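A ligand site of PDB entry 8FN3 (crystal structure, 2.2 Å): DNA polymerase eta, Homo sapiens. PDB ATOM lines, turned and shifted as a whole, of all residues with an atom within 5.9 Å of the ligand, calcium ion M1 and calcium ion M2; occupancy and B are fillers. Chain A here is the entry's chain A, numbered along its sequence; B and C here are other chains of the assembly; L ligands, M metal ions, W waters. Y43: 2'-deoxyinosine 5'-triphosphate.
An oxygen (OAH) of the ligand sits close to O3' of DG 8 of chain C (3.2 Å).
CA of Asp 15 touches OAS of the ligand (3.5 Å).
O of Ile 48 touches CAC of the ligand, at 3.5 Å.
Ala 49 touches the ligand (CB to OAA, 3.6 Å).
DT 3 of chain B touches the ligand.
DC 5 of chain B touches the ligand.
Hydrophobic or aromatic side chains that line the ligand: Phe 17, Phe 18, Ile 48, Ala 49 and Tyr 52.
17 residues have an atom within 4 Å of the ligand: Asp 13, Met 14, Asp 15, Cys 16, Phe 17, Phe 18, Ile 48, Ala 49, Tyr 52, Arg 55, Arg 61, Asp 115, Lys 231, DT 3 of chain B, DC 4 of chain B, DC 5 of chain B and DG 8 of chain C.
The nearest printed residue that does not touch the ligand is Ile 114 (4.2 Å).
Calcium ion M1 is bound by the side-chain carboxylate (OD1) of Asp 13 (2.2 Å), the side-chain carboxylate (OD2) of Asp 115 (2.2 Å), the backbone carbonyl oxygen (O) of Met 14 (2.3 Å), an oxygen (OAR) of the ligand (2.4 Å), an oxygen (OAN) of the ligand (2.4 Å) and an oxygen (OAK) of the ligand (2.6 Å).
N1 of the ligand lies close to N3 of DC 4 of chain B (2.5 Å).
The side-chain hydroxyl (OH) of Tyr 52 is in hydrogen-bond range of an oxygen (OAS) of the ligand, at 2.6 Å.
The guanidinium group (NH1) of Arg 55 lies within salt-bridge range of an oxygen (OAT) of the ligand (3.0 Å).
The backbone NH of Cys 16 sits at hydrogen-bond distance from an oxygen (OAS) of the ligand.
OAA of the ligand sits at hydrogen-bond distance from N of Phe 17 (3.4 Å).
NH2 of Arg 61 is in salt-bridge range of OAO of the ligand (3.1 Å).
N of Phe 18 lies within hydrogen-bond range of OAA of the ligand, at 3.2 Å.
An oxygen (OAS) of the ligand lies within salt-bridge range of the side-chain amino group (NZ) of Lys 231, at 3.8 Å.
The side-chain amino group (NZ) of Lys 231 sits close to the side-chain carboxylate (OD2) of Asp 13 (3.8 Å).
OG of Ser 113 sits close to N of Glu 116 (3.3 Å).
OE2 of Glu 116 is in salt-bridge range of NZ of Lys 224 (2.7 Å).
O2 of DC 4 of chain B sits at hydrogen-bond distance from the side-chain amide nitrogen (NE2) of Gln 38 (2.7 Å).
The backbone carbonyl oxygen (O) of Val 50 sits at hydrogen-bond distance from the guanidinium group (NE) of Arg 55 (2.8 Å).
O of Ile 48 sits at hydrogen-bond distance from NE of Arg 61 (3.1 Å).
O2 of DC 5 of chain B lies close to N2 of DG 8 of chain C (2.6 Å).
The side-chain hydroxyl of Ser 113 is in hydrogen-bond range of O3' of DG 8 of chain C (2.9 Å).
Calcium ion M2 is bound by an oxygen (OAK) of the ligand, the side-chain carboxylate (OE1) of Glu 116, the side-chain carboxylate (OD1) of Asp 13, the side-chain carboxylate (OD2) of Asp 13 and the side-chain carboxylate (OD1) of Asp 115.
Three residues have an atom within 4 Å of calcium ion M1: Asp 13, Met 14 and Asp 115.
DG 8 of chain C touches calcium ion M2.
Four residues have an atom within 4 Å of calcium ion M2: Asp 13, Asp 115, Glu 116 and DG 8 of chain C.
The nearest printed residue that does not touch calcium ion M2 is Ser 113 (4.5 Å).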
ATOM      1  N   ASP A  13      -1.067   1.662  -2.835  1.00  0.00           N
ATOM      2  CA  ASP A  13       0.304   1.214  -3.075  1.00  0.00           C
ATOM      3  C   ASP A  13       1.250   2.315  -2.654  1.00  0.00           C
ATOM      4  O   ASP A  13       1.270   3.391  -3.265  1.00  0.00           O
ATOM      5  CB  ASP A  13       0.509   0.886  -4.561  1.00  0.00           C
ATOM      6  CG  ASP A  13       1.814   0.171  -4.843  1.00  0.00           C
ATOM      7  OD1 ASP A  13       2.748   0.254  -4.021  1.00  0.00           O
ATOM      8  OD2 ASP A  13       1.928  -0.436  -5.923  1.00  0.00           O
ATOM      9  N   MET A  14       2.066   2.056  -1.625  1.00  0.00           N
ATOM     10  CA  MET A  14       3.001   3.080  -1.182  1.00  0.00           C
ATOM     11  C   MET A  14       4.078   3.343  -2.234  1.00  0.00           C
ATOM     12  O   MET A  14       4.657   2.419  -2.803  1.00  0.00           O
ATOM     13  CB  MET A  14       3.598   2.687   0.182  1.00  0.00           C
ATOM     14  CG  MET A  14       2.619   1.907   1.092  1.00  0.00           C
ATOM     15  SD  MET A  14       1.477   3.173   1.723  1.00  0.00           S
ATOM     16  CE  MET A  14       2.788   4.285   2.177  1.00  0.00           C
ATOM     17  N   ASP A  15       4.313   4.631  -2.510  1.00  0.00           N
ATOM     18  CA  ASP A  15       5.334   5.056  -3.461  1.00  0.00           C
ATOM     19  C   ASP A  15       6.713   4.718  -2.925  1.00  0.00           C
ATOM     20  O   ASP A  15       7.036   5.075  -1.785  1.00  0.00           O
ATOM     21  CB  ASP A  15       5.209   6.554  -3.742  1.00  0.00           C
ATOM     22  CG  ASP A  15       3.848   6.923  -4.330  1.00  0.00           C
ATOM     23  OD1 ASP A  15       3.260   6.078  -5.015  1.00  0.00           O
ATOM     24  OD2 ASP A  15       3.357   8.043  -4.087  1.00  0.00           O
ATOM     25  N   CYS A  16       7.517   4.033  -3.746  1.00  0.00           N
ATOM     26  CA  CYS A  16       8.858   3.551  -3.416  1.00  0.00           C
ATOM     27  C   CYS A  16       9.050   3.297  -1.924  1.00  0.00           C
ATOM     28  O   CYS A  16       9.796   4.033  -1.263  1.00  0.00           O
ATOM     29  CB  CYS A  16       9.910   4.533  -3.917  1.00  0.00           C
ATOM     30  SG  CYS A  16       9.640   6.254  -3.405  1.00  0.00           S
ATOM     31  N   PHE A  17       8.433   2.248  -1.401  1.00  0.00           N
ATOM     32  CA  PHE A  17       8.144   2.180   0.034  1.00  0.00           C
ATOM     33  C   PHE A  17       9.402   2.164   0.901  1.00  0.00           C
ATOM     34  O   PHE A  17       9.526   2.973   1.842  1.00  0.00           O
ATOM     35  CB  PHE A  17       7.301   0.943   0.334  1.00  0.00           C
ATOM     36  CG  PHE A  17       6.899   0.832   1.755  1.00  0.00           C
ATOM     37  CD1 PHE A  17       6.465   1.958   2.439  1.00  0.00           C
ATOM     38  CD2 PHE A  17       6.968  -0.380   2.425  1.00  0.00           C
ATOM     39  CE1 PHE A  17       6.093   1.882   3.764  1.00  0.00           C
ATOM     40  CE2 PHE A  17       6.570  -0.462   3.769  1.00  0.00           C
ATOM     41  CZ  PHE A  17       6.148   0.659   4.419  1.00  0.00           C
ATOM     42  N   PHE A  18      10.322   1.225   0.658  1.00  0.00           N
ATOM     43  CA  PHE A  18      11.494   1.142   1.533  1.00  0.00           C
ATOM     44  C   PHE A  18      12.254   2.466   1.536  1.00  0.00           C
ATOM     45  O   PHE A  18      12.746   2.899   2.586  1.00  0.00           O
ATOM     46  CB  PHE A  18      12.394  -0.014   1.105  1.00  0.00           C
ATOM     47  CG  PHE A  18      11.836  -1.373   1.447  1.00  0.00           C
ATOM     48  CD1 PHE A  18      10.478  -1.547   1.658  1.00  0.00           C
ATOM     49  CD2 PHE A  18      12.670  -2.471   1.549  1.00  0.00           C
ATOM     50  CE1 PHE A  18       9.947  -2.789   1.968  1.00  0.00           C
ATOM     51  CE2 PHE A  18      12.166  -3.733   1.857  1.00  0.00           C
ATOM     52  CZ  PHE A  18      10.791  -3.885   2.080  1.00  0.00           C
ATOM     53  N   VAL A  19      12.344   3.127   0.377  1.00  0.00           N
ATOM     54  CA  VAL A  19      13.020   4.427   0.275  1.00  0.00           C
ATOM     55  C   VAL A  19      12.343   5.448   1.193  1.00  0.00           C
ATOM     56  O   VAL A  19      13.007   6.130   1.981  1.00  0.00           O
ATOM     57  CB  VAL A  19      13.048   4.911  -1.194  1.00  0.00           C
ATOM     58  CG1 VAL A  19      13.424   6.371  -1.277  1.00  0.00           C
ATOM     59  CG2 VAL A  19      14.034   4.075  -2.013  1.00  0.00           C
ATOM     60  N   GLN A  38      20.787  -3.891  -0.023  1.00  0.00           N
ATOM     61  CA  GLN A  38      21.199  -4.860   1.003  1.00  0.00           C
ATOM     62  C   GLN A  38      22.528  -5.499   0.640  1.00  0.00           C
ATOM     63  O   GLN A  38      22.812  -5.776  -0.529  1.00  0.00           O
ATOM     64  CB  GLN A  38      20.138  -5.940   1.220  1.00  0.00           C
ATOM     65  CG  GLN A  38      19.733  -6.742   0.009  1.00  0.00           C
ATOM     66  CD  GLN A  38      18.550  -7.631   0.316  1.00  0.00           C
ATOM     67  OE1 GLN A  38      17.879  -7.447   1.328  1.00  0.00           O
ATOM     68  NE2 GLN A  38      18.294  -8.594  -0.531  1.00  0.00           N
ATOM     69  N   ILE A  48      17.125  -2.633  -3.936  1.00  0.00           N
ATOM     70  CA  ILE A  48      15.773  -3.152  -3.816  1.00  0.00           C
ATOM     71  C   ILE A  48      14.693  -2.078  -3.864  1.00  0.00           C
ATOM     72  O   ILE A  48      13.512  -2.438  -3.968  1.00  0.00           O
ATOM     73  CB  ILE A  48      15.621  -4.025  -2.548  1.00  0.00           C
ATOM     74  CG1 ILE A  48      16.054  -3.280  -1.287  1.00  0.00           C
ATOM     75  CG2 ILE A  48      16.382  -5.329  -2.694  1.00  0.00           C
ATOM     76  CD1 ILE A  48      15.643  -3.993  -0.036  1.00  0.00           C
ATOM     77  N   ALA A  49      15.043  -0.788  -3.859  1.00  0.00           N
ATOM     78  CA  ALA A  49      14.043   0.256  -3.900  1.00  0.00           C
ATOM     79  C   ALA A  49      14.706   1.565  -4.291  1.00  0.00           C
ATOM     80  O   ALA A  49      15.833   1.837  -3.865  1.00  0.00           O
ATOM     81  CB  ALA A  49      13.320   0.404  -2.552  1.00  0.00           C
ATOM     82  N   VAL A  50      14.000   2.370  -5.083  1.00  0.00           N
ATOM     83  CA  VAL A  50      14.593   3.508  -5.787  1.00  0.00           C
ATOM     84  C   VAL A  50      13.619   4.679  -5.734  1.00  0.00           C
ATOM     85  O   VAL A  50      12.497   4.585  -6.248  1.00  0.00           O
ATOM     86  CB  VAL A  50      14.904   3.175  -7.260  1.00  0.00           C
ATOM     87  CG1 VAL A  50      15.765   4.253  -7.878  1.00  0.00           C
ATOM     88  CG2 VAL A  50      15.558   1.827  -7.403  1.00  0.00           C
ATOM     89  N   TYR A  52      11.954   8.311  -6.718  1.00  0.00           N
ATOM     90  CA  TYR A  52      11.598   8.751  -8.060  1.00  0.00           C
ATOM     91  C   TYR A  52      12.626   9.693  -8.653  1.00  0.00           C
ATOM     92  O   TYR A  52      12.777   9.734  -9.883  1.00  0.00           O
ATOM     93  CB  TYR A  52      10.209   9.370  -8.065  1.00  0.00           C
ATOM     94  CG  TYR A  52       9.171   8.296  -8.112  1.00  0.00           C
ATOM     95  CD1 TYR A  52       8.853   7.586  -6.976  1.00  0.00           C
ATOM     96  CD2 TYR A  52       8.580   7.924  -9.305  1.00  0.00           C
ATOM     97  CE1 TYR A  52       7.947   6.568  -7.002  1.00  0.00           C
ATOM     98  CE2 TYR A  52       7.654   6.892  -9.338  1.00  0.00           C
ATOM     99  CZ  TYR A  52       7.339   6.219  -8.184  1.00  0.00           C
ATOM    100  OH  TYR A  52       6.415   5.174  -8.182  1.00  0.00           O
ATOM    101  N   ARG A  55      15.155   7.337 -10.194  1.00  0.00           N
ATOM    102  CA  ARG A  55      14.631   6.660 -11.385  1.00  0.00           C
ATOM    103  C   ARG A  55      14.831   7.490 -12.650  1.00  0.00           C
ATOM    104  O   ARG A  55      15.061   6.939 -13.735  1.00  0.00           O
ATOM    105  CB  ARG A  55      13.159   6.324 -11.217  1.00  0.00           C
ATOM    106  CG  ARG A  55      12.857   5.324 -10.113  1.00  0.00           C
ATOM    107  CD  ARG A  55      11.356   4.927 -10.024  1.00  0.00           C
ATOM    108  NE  ARG A  55      11.056   4.401  -8.692  1.00  0.00           N
ATOM    109  CZ  ARG A  55       9.962   3.715  -8.369  1.00  0.00           C
ATOM    110  NH1 ARG A  55       9.023   3.439  -9.259  1.00  0.00           N
ATOM    111  NH2 ARG A  55       9.823   3.297  -7.118  1.00  0.00           N
ATOM    112  N   ARG A  61      15.611  -1.272  -9.632  1.00  0.00           N
ATOM    113  CA  ARG A  61      15.770  -2.425  -8.768  1.00  0.00           C
ATOM    114  C   ARG A  61      16.615  -3.500  -9.459  1.00  0.00           C
ATOM    115  O   ARG A  61      16.724  -3.544 -10.695  1.00  0.00           O
ATOM    116  CB  ARG A  61      14.395  -2.949  -8.384  1.00  0.00           C
ATOM    117  CG  ARG A  61      14.339  -4.201  -7.587  1.00  0.00           C
ATOM    118  CD  ARG A  61      12.890  -4.610  -7.435  1.00  0.00           C
ATOM    119  NE  ARG A  61      12.235  -3.786  -6.431  1.00  0.00           N
ATOM    120  CZ  ARG A  61      11.209  -2.979  -6.645  1.00  0.00           C
ATOM    121  NH1 ARG A  61      10.622  -2.911  -7.830  1.00  0.00           N
ATOM    122  NH2 ARG A  61      10.751  -2.229  -5.644  1.00  0.00           N
ATOM    123  N   LEU A  89      14.472  -7.283   7.768  1.00  0.00           N
ATOM    124  CA  LEU A  89      13.462  -6.407   7.206  1.00  0.00           C
ATOM    125  C   LEU A  89      12.530  -5.788   8.263  1.00  0.00           C
ATOM    126  O   LEU A  89      11.503  -5.204   7.900  1.00  0.00           O
ATOM    127  CB  LEU A  89      12.644  -7.198   6.179  1.00  0.00           C
ATOM    128  CG  LEU A  89      13.323  -7.633   4.877  1.00  0.00           C
ATOM    129  CD1 LEU A  89      12.256  -7.807   3.798  1.00  0.00           C
ATOM    130  CD2 LEU A  89      14.362  -6.588   4.436  1.00  0.00           C
ATOM    131  N   SER A 113       0.736  -7.389  -0.104  1.00  0.00           N
ATOM    132  CA  SER A 113       2.197  -7.400  -0.053  1.00  0.00           C
ATOM    133  C   SER A 113       2.593  -6.493   1.107  1.00  0.00           C
ATOM    134  O   SER A 113       1.735  -5.914   1.782  1.00  0.00           O
ATOM    135  CB  SER A 113       2.803  -6.929  -1.374  1.00  0.00           C
ATOM    136  OG  SER A 113       2.847  -5.510  -1.411  1.00  0.00           O
ATOM    137  N   ILE A 114       3.902  -6.381   1.355  1.00  0.00           N
ATOM    138  CA  ILE A 114       4.324  -5.538   2.451  1.00  0.00           C
ATOM    139  C   ILE A 114       3.811  -4.109   2.296  1.00  0.00           C
ATOM    140  O   ILE A 114       3.636  -3.415   3.300  1.00  0.00           O
ATOM    141  CB  ILE A 114       5.855  -5.568   2.602  1.00  0.00           C
ATOM    142  CG1 ILE A 114       6.238  -5.000   3.970  1.00  0.00           C
ATOM    143  CG2 ILE A 114       6.514  -4.773   1.462  1.00  0.00           C
ATOM    144  CD1 ILE A 114       7.690  -5.134   4.281  1.00  0.00           C
ATOM    145  N   ASP A 115       3.524  -3.659   1.066  1.00  0.00           N
ATOM    146  CA  ASP A 115       3.205  -2.241   0.894  1.00  0.00           C
ATOM    147  C   ASP A 115       1.966  -1.974   0.041  1.00  0.00           C
ATOM    148  O   ASP A 115       1.791  -0.849  -0.443  1.00  0.00           O
ATOM    149  CB  ASP A 115       4.412  -1.508   0.315  1.00  0.00           C
ATOM    150  CG  ASP A 115       4.440  -1.550  -1.186  1.00  0.00           C
ATOM    151  OD1 ASP A 115       4.155  -2.637  -1.762  1.00  0.00           O
ATOM    152  OD2 ASP A 115       4.745  -0.492  -1.774  1.00  0.00           O
ATOM    153  N   GLU A 116       1.086  -2.963  -0.141  1.00  0.00           N
ATOM    154  CA  GLU A 116      -0.158  -2.685  -0.831  1.00  0.00           C
ATOM    155  C   GLU A 116      -1.252  -3.564  -0.260  1.00  0.00           C
ATOM    156  O   GLU A 116      -1.021  -4.691   0.185  1.00  0.00           O
ATOM    157  CB  GLU A 116      -0.065  -2.891  -2.346  1.00  0.00           C
ATOM    158  CG  GLU A 116       0.070  -4.296  -2.812  1.00  0.00           C
ATOM    159  CD  GLU A 116       0.797  -4.358  -4.157  1.00  0.00           C
ATOM    160  OE1 GLU A 116       2.026  -4.228  -4.179  1.00  0.00           O
ATOM    161  OE2 GLU A 116       0.140  -4.527  -5.197  1.00  0.00           O
ATOM    162  N   LYS A 224      -5.580  -2.472  -9.553  1.00  0.00           N
ATOM    163  CA  LYS A 224      -4.128  -2.556  -9.556  1.00  0.00           C
ATOM    164  C   LYS A 224      -3.531  -1.908 -10.801  1.00  0.00           C
ATOM    165  O   LYS A 224      -2.535  -1.171 -10.730  1.00  0.00           O
ATOM    166  CB  LYS A 224      -3.715  -4.029  -9.473  1.00  0.00           C
ATOM    167  CG  LYS A 224      -2.389  -4.244  -8.784  1.00  0.00           C
ATOM    168  CD  LYS A 224      -1.274  -4.509  -9.759  1.00  0.00           C
ATOM    169  CE  LYS A 224      -0.021  -4.999  -9.028  1.00  0.00           C
ATOM    170  NZ  LYS A 224       0.374  -4.120  -7.882  1.00  0.00           N
ATOM    171  N   LYS A 231       1.555   7.441 -11.156  1.00  0.00           N
ATOM    172  CA  LYS A 231       2.344   7.549  -9.934  1.00  0.00           C
ATOM    173  C   LYS A 231       3.456   8.581 -10.107  1.00  0.00           C
ATOM    174  O   LYS A 231       3.883   8.841 -11.235  1.00  0.00           O
ATOM    175  CB  LYS A 231       2.970   6.205  -9.542  1.00  0.00           C
ATOM    176  CG  LYS A 231       2.209   4.944  -9.895  1.00  0.00           C
ATOM    177  CD  LYS A 231       3.091   3.704  -9.795  1.00  0.00           C
ATOM    178  CE  LYS A 231       3.737   3.568  -8.420  1.00  0.00           C
ATOM    179  NZ  LYS A 231       2.803   2.914  -7.456  1.00  0.00           N
ATOM    180  P    DT B   3      22.019 -11.105 -10.247  1.00  0.00           P
ATOM    181  OP1  DT B   3      21.117 -12.288 -10.240  1.00  0.00           O
ATOM    182  OP2  DT B   3      22.691 -10.681 -11.498  1.00  0.00           O
ATOM    183  O5'  DT B   3      21.165  -9.838  -9.676  1.00  0.00           O
ATOM    184  C5'  DT B   3      21.682  -8.944  -8.658  1.00  0.00           C
ATOM    185  C4'  DT B   3      21.063  -9.266  -7.289  1.00  0.00           C
ATOM    186  O4'  DT B   3      19.875  -8.445  -7.081  1.00  0.00           O
ATOM    187  C3'  DT B   3      20.629 -10.732  -7.118  1.00  0.00           C
ATOM    188  O3'  DT B   3      20.963 -11.214  -5.814  1.00  0.00           O
ATOM    189  C2'  DT B   3      19.114 -10.666  -7.308  1.00  0.00           C
ATOM    190  C1'  DT B   3      18.778  -9.287  -6.753  1.00  0.00           C
ATOM    191  N1   DT B   3      17.479  -8.728  -7.312  1.00  0.00           N
ATOM    192  C2   DT B   3      16.847  -7.675  -6.669  1.00  0.00           C
ATOM    193  O2   DT B   3      17.317  -7.120  -5.673  1.00  0.00           O
ATOM    194  N3   DT B   3      15.669  -7.263  -7.256  1.00  0.00           N
ATOM    195  C4   DT B   3      15.051  -7.809  -8.391  1.00  0.00           C
ATOM    196  O4   DT B   3      13.983  -7.368  -8.839  1.00  0.00           O
ATOM    197  C5   DT B   3      15.763  -8.935  -9.006  1.00  0.00           C
ATOM    198  C7   DT B   3      15.200  -9.614 -10.229  1.00  0.00           C
ATOM    199  C6   DT B   3      16.915  -9.323  -8.440  1.00  0.00           C
ATOM    200  P    DC B   4      21.516 -12.723  -5.584  1.00  0.00           P
ATOM    201  OP1  DC B   4      22.816 -12.827  -6.284  1.00  0.00           O
ATOM    202  OP2  DC B   4      20.481 -13.741  -5.886  1.00  0.00           O
ATOM    203  O5'  DC B   4      21.810 -12.703  -4.003  1.00  0.00           O
ATOM    204  C5'  DC B   4      21.867 -11.433  -3.315  1.00  0.00           C
ATOM    205  C4'  DC B   4      20.695 -11.259  -2.346  1.00  0.00           C
ATOM    206  O4'  DC B   4      19.575 -10.635  -3.005  1.00  0.00           O
ATOM    207  C3'  DC B   4      20.159 -12.555  -1.714  1.00  0.00           C
ATOM    208  O3'  DC B   4      20.305 -12.464  -0.324  1.00  0.00           O
ATOM    209  C2'  DC B   4      18.677 -12.601  -2.134  1.00  0.00           C
ATOM    210  C1'  DC B   4      18.377 -11.151  -2.465  1.00  0.00           C
ATOM    211  N1   DC B   4      17.232 -10.938  -3.461  1.00  0.00           N
ATOM    212  C2   DC B   4      16.182 -10.053  -3.156  1.00  0.00           C
ATOM    213  O2   DC B   4      16.200  -9.447  -2.082  1.00  0.00           O
ATOM    214  N3   DC B   4      15.187  -9.873  -4.050  1.00  0.00           N
ATOM    215  C4   DC B   4      15.185 -10.547  -5.197  1.00  0.00           C
ATOM    216  N4   DC B   4      14.164 -10.331  -6.041  1.00  0.00           N
ATOM    217  C5   DC B   4      16.222 -11.454  -5.536  1.00  0.00           C
ATOM    218  C6   DC B   4      17.218 -11.617  -4.647  1.00  0.00           C
ATOM    219  P    DC B   5      19.708 -13.564   0.665  1.00  0.00           P
ATOM    220  OP1  DC B   5      20.448 -13.389   1.922  1.00  0.00           O
ATOM    221  OP2  DC B   5      19.555 -14.897   0.035  1.00  0.00           O
ATOM    222  O5'  DC B   5      18.224 -13.040   0.921  1.00  0.00           O
ATOM    223  C5'  DC B   5      18.034 -11.871   1.665  1.00  0.00           C
ATOM    224  C4'  DC B   5      16.574 -11.533   1.744  1.00  0.00           C
ATOM    225  O4'  DC B   5      16.022 -11.426   0.402  1.00  0.00           O
ATOM    226  C3'  DC B   5      15.728 -12.598   2.460  1.00  0.00           C
ATOM    227  O3'  DC B   5      14.936 -11.937   3.415  1.00  0.00           O
ATOM    228  C2'  DC B   5      14.881 -13.198   1.325  1.00  0.00           C
ATOM    229  C1'  DC B   5      14.738 -11.981   0.436  1.00  0.00           C
ATOM    230  N1   DC B   5      14.308 -12.268  -0.929  1.00  0.00           N
ATOM    231  C2   DC B   5      13.240 -11.545  -1.447  1.00  0.00           C
ATOM    232  O2   DC B   5      12.708 -10.695  -0.727  1.00  0.00           O
ATOM    233  N3   DC B   5      12.825 -11.790  -2.700  1.00  0.00           N
ATOM    234  C4   DC B   5      13.445 -12.700  -3.447  1.00  0.00           C
ATOM    235  N4   DC B   5      12.987 -12.903  -4.687  1.00  0.00           N
ATOM    236  C5   DC B   5      14.559 -13.457  -2.937  1.00  0.00           C
ATOM    237  C6   DC B   5      14.955 -13.198  -1.678  1.00  0.00           C
ATOM    238  P    DG C   8       4.148  -6.651  -8.699  1.00  0.00           P
ATOM    239  OP1  DG C   8       3.214  -5.542  -8.982  1.00  0.00           O
ATOM    240  OP2  DG C   8       5.383  -6.823  -9.522  1.00  0.00           O
ATOM    241  O5'  DG C   8       4.563  -6.530  -7.152  1.00  0.00           O
ATOM    242  C5'  DG C   8       3.588  -6.666  -6.109  1.00  0.00           C
ATOM    243  C4'  DG C   8       4.262  -6.641  -4.758  1.00  0.00           C
ATOM    244  O4'  DG C   8       5.033  -7.864  -4.561  1.00  0.00           O
ATOM    245  C3'  DG C   8       5.213  -5.459  -4.538  1.00  0.00           C
ATOM    246  O3'  DG C   8       4.912  -4.765  -3.320  1.00  0.00           O
ATOM    247  C2'  DG C   8       6.618  -6.073  -4.478  1.00  0.00           C
ATOM    248  C1'  DG C   8       6.378  -7.569  -4.211  1.00  0.00           C
ATOM    249  N9   DG C   8       7.292  -8.425  -4.988  1.00  0.00           N
ATOM    250  C8   DG C   8       7.253  -8.679  -6.343  1.00  0.00           C
ATOM    251  N7   DG C   8       8.237  -9.443  -6.751  1.00  0.00           N
ATOM    252  C5   DG C   8       8.994  -9.683  -5.597  1.00  0.00           C
ATOM    253  C6   DG C   8      10.193 -10.446  -5.416  1.00  0.00           C
ATOM    254  O6   DG C   8      10.847 -11.087  -6.267  1.00  0.00           O
ATOM    255  N1   DG C   8      10.620 -10.418  -4.081  1.00  0.00           N
ATOM    256  C2   DG C   8       9.972  -9.747  -3.063  1.00  0.00           C
ATOM    257  N2   DG C   8      10.525  -9.819  -1.839  1.00  0.00           N
ATOM    258  N3   DG C   8       8.851  -9.048  -3.226  1.00  0.00           N
ATOM    259  C4   DG C   8       8.428  -9.053  -4.507  1.00  0.00           C
HETATM  260  C4  Y43 L   1      11.882  -6.105  -2.646  1.00  0.00           C
HETATM  261  C5  Y43 L   1      11.919  -6.700  -3.848  1.00  0.00           C
HETATM  262  C6  Y43 L   1      12.855  -7.633  -4.089  1.00  0.00           C
HETATM  263  C8  Y43 L   1      10.312  -5.246  -3.884  1.00  0.00           C
HETATM  264  N1  Y43 L   1      13.783  -8.012  -3.084  1.00  0.00           N
HETATM  265  N3  Y43 L   1      12.738  -6.446  -1.680  1.00  0.00           N
HETATM  266  C2  Y43 L   1      13.714  -7.441  -1.905  1.00  0.00           C
HETATM  267  CAB Y43 L   1       9.943  -2.185  -2.164  1.00  0.00           C
HETATM  268  CAC Y43 L   1      11.090  -2.945  -1.507  1.00  0.00           C
HETATM  269  CAD Y43 L   1      10.489  -4.359  -1.510  1.00  0.00           C
HETATM  270  CAF Y43 L   1       8.779  -2.819  -1.477  1.00  0.00           C
HETATM  271  CAG Y43 L   1       7.511  -2.495  -2.272  1.00  0.00           C
HETATM  272  N7  Y43 L   1      10.959  -6.164  -4.614  1.00  0.00           N
HETATM  273  N9  Y43 L   1      10.884  -5.218  -2.666  1.00  0.00           N
HETATM  274  O6  Y43 L   1      12.915  -8.187  -5.199  1.00  0.00           O
HETATM  275  OAA Y43 L   1       9.974  -0.799  -1.834  1.00  0.00           O
HETATM  276  OAE Y43 L   1       9.086  -4.174  -1.772  1.00  0.00           O
HETATM  277  OAH Y43 L   1       7.642  -3.071  -3.595  1.00  0.00           O
HETATM  278  OAJ Y43 L   1       7.151  -3.439  -6.157  1.00  0.00           O
HETATM  279  OAK Y43 L   1       5.613  -1.934  -4.747  1.00  0.00           O
HETATM  280  OAL Y43 L   1       7.980  -1.134  -5.513  1.00  0.00           O
HETATM  281  OAN Y43 L   1       7.278   0.495  -3.486  1.00  0.00           O
HETATM  282  OAO Y43 L   1       9.720   0.352  -4.235  1.00  0.00           O
HETATM  283  OAP Y43 L   1       8.078   1.493  -5.828  1.00  0.00           O
HETATM  284  OAR Y43 L   1       5.425   1.052  -6.063  1.00  0.00           O
HETATM  285  OAS Y43 L   1       6.404   3.423  -6.313  1.00  0.00           O
HETATM  286  OAT Y43 L   1       6.904   1.569  -8.117  1.00  0.00           O
HETATM  287  PAI Y43 L   1       7.005  -2.377  -4.968  1.00  0.00           P
HETATM  288  PAM Y43 L   1       8.308   0.262  -4.730  1.00  0.00           P
HETATM  289  PAQ Y43 L   1       6.716   1.862  -6.662  1.00  0.00           P
HETATM  290 CA    CA M   1       4.910   0.350  -3.832  1.00  0.00          CA
HETATM  291 CA    CA M   2       3.379  -2.262  -4.479  1.00  0.00          CA
HETATM  292  O   HOH W   1      11.762   1.036  -6.014  1.00  0.00           O
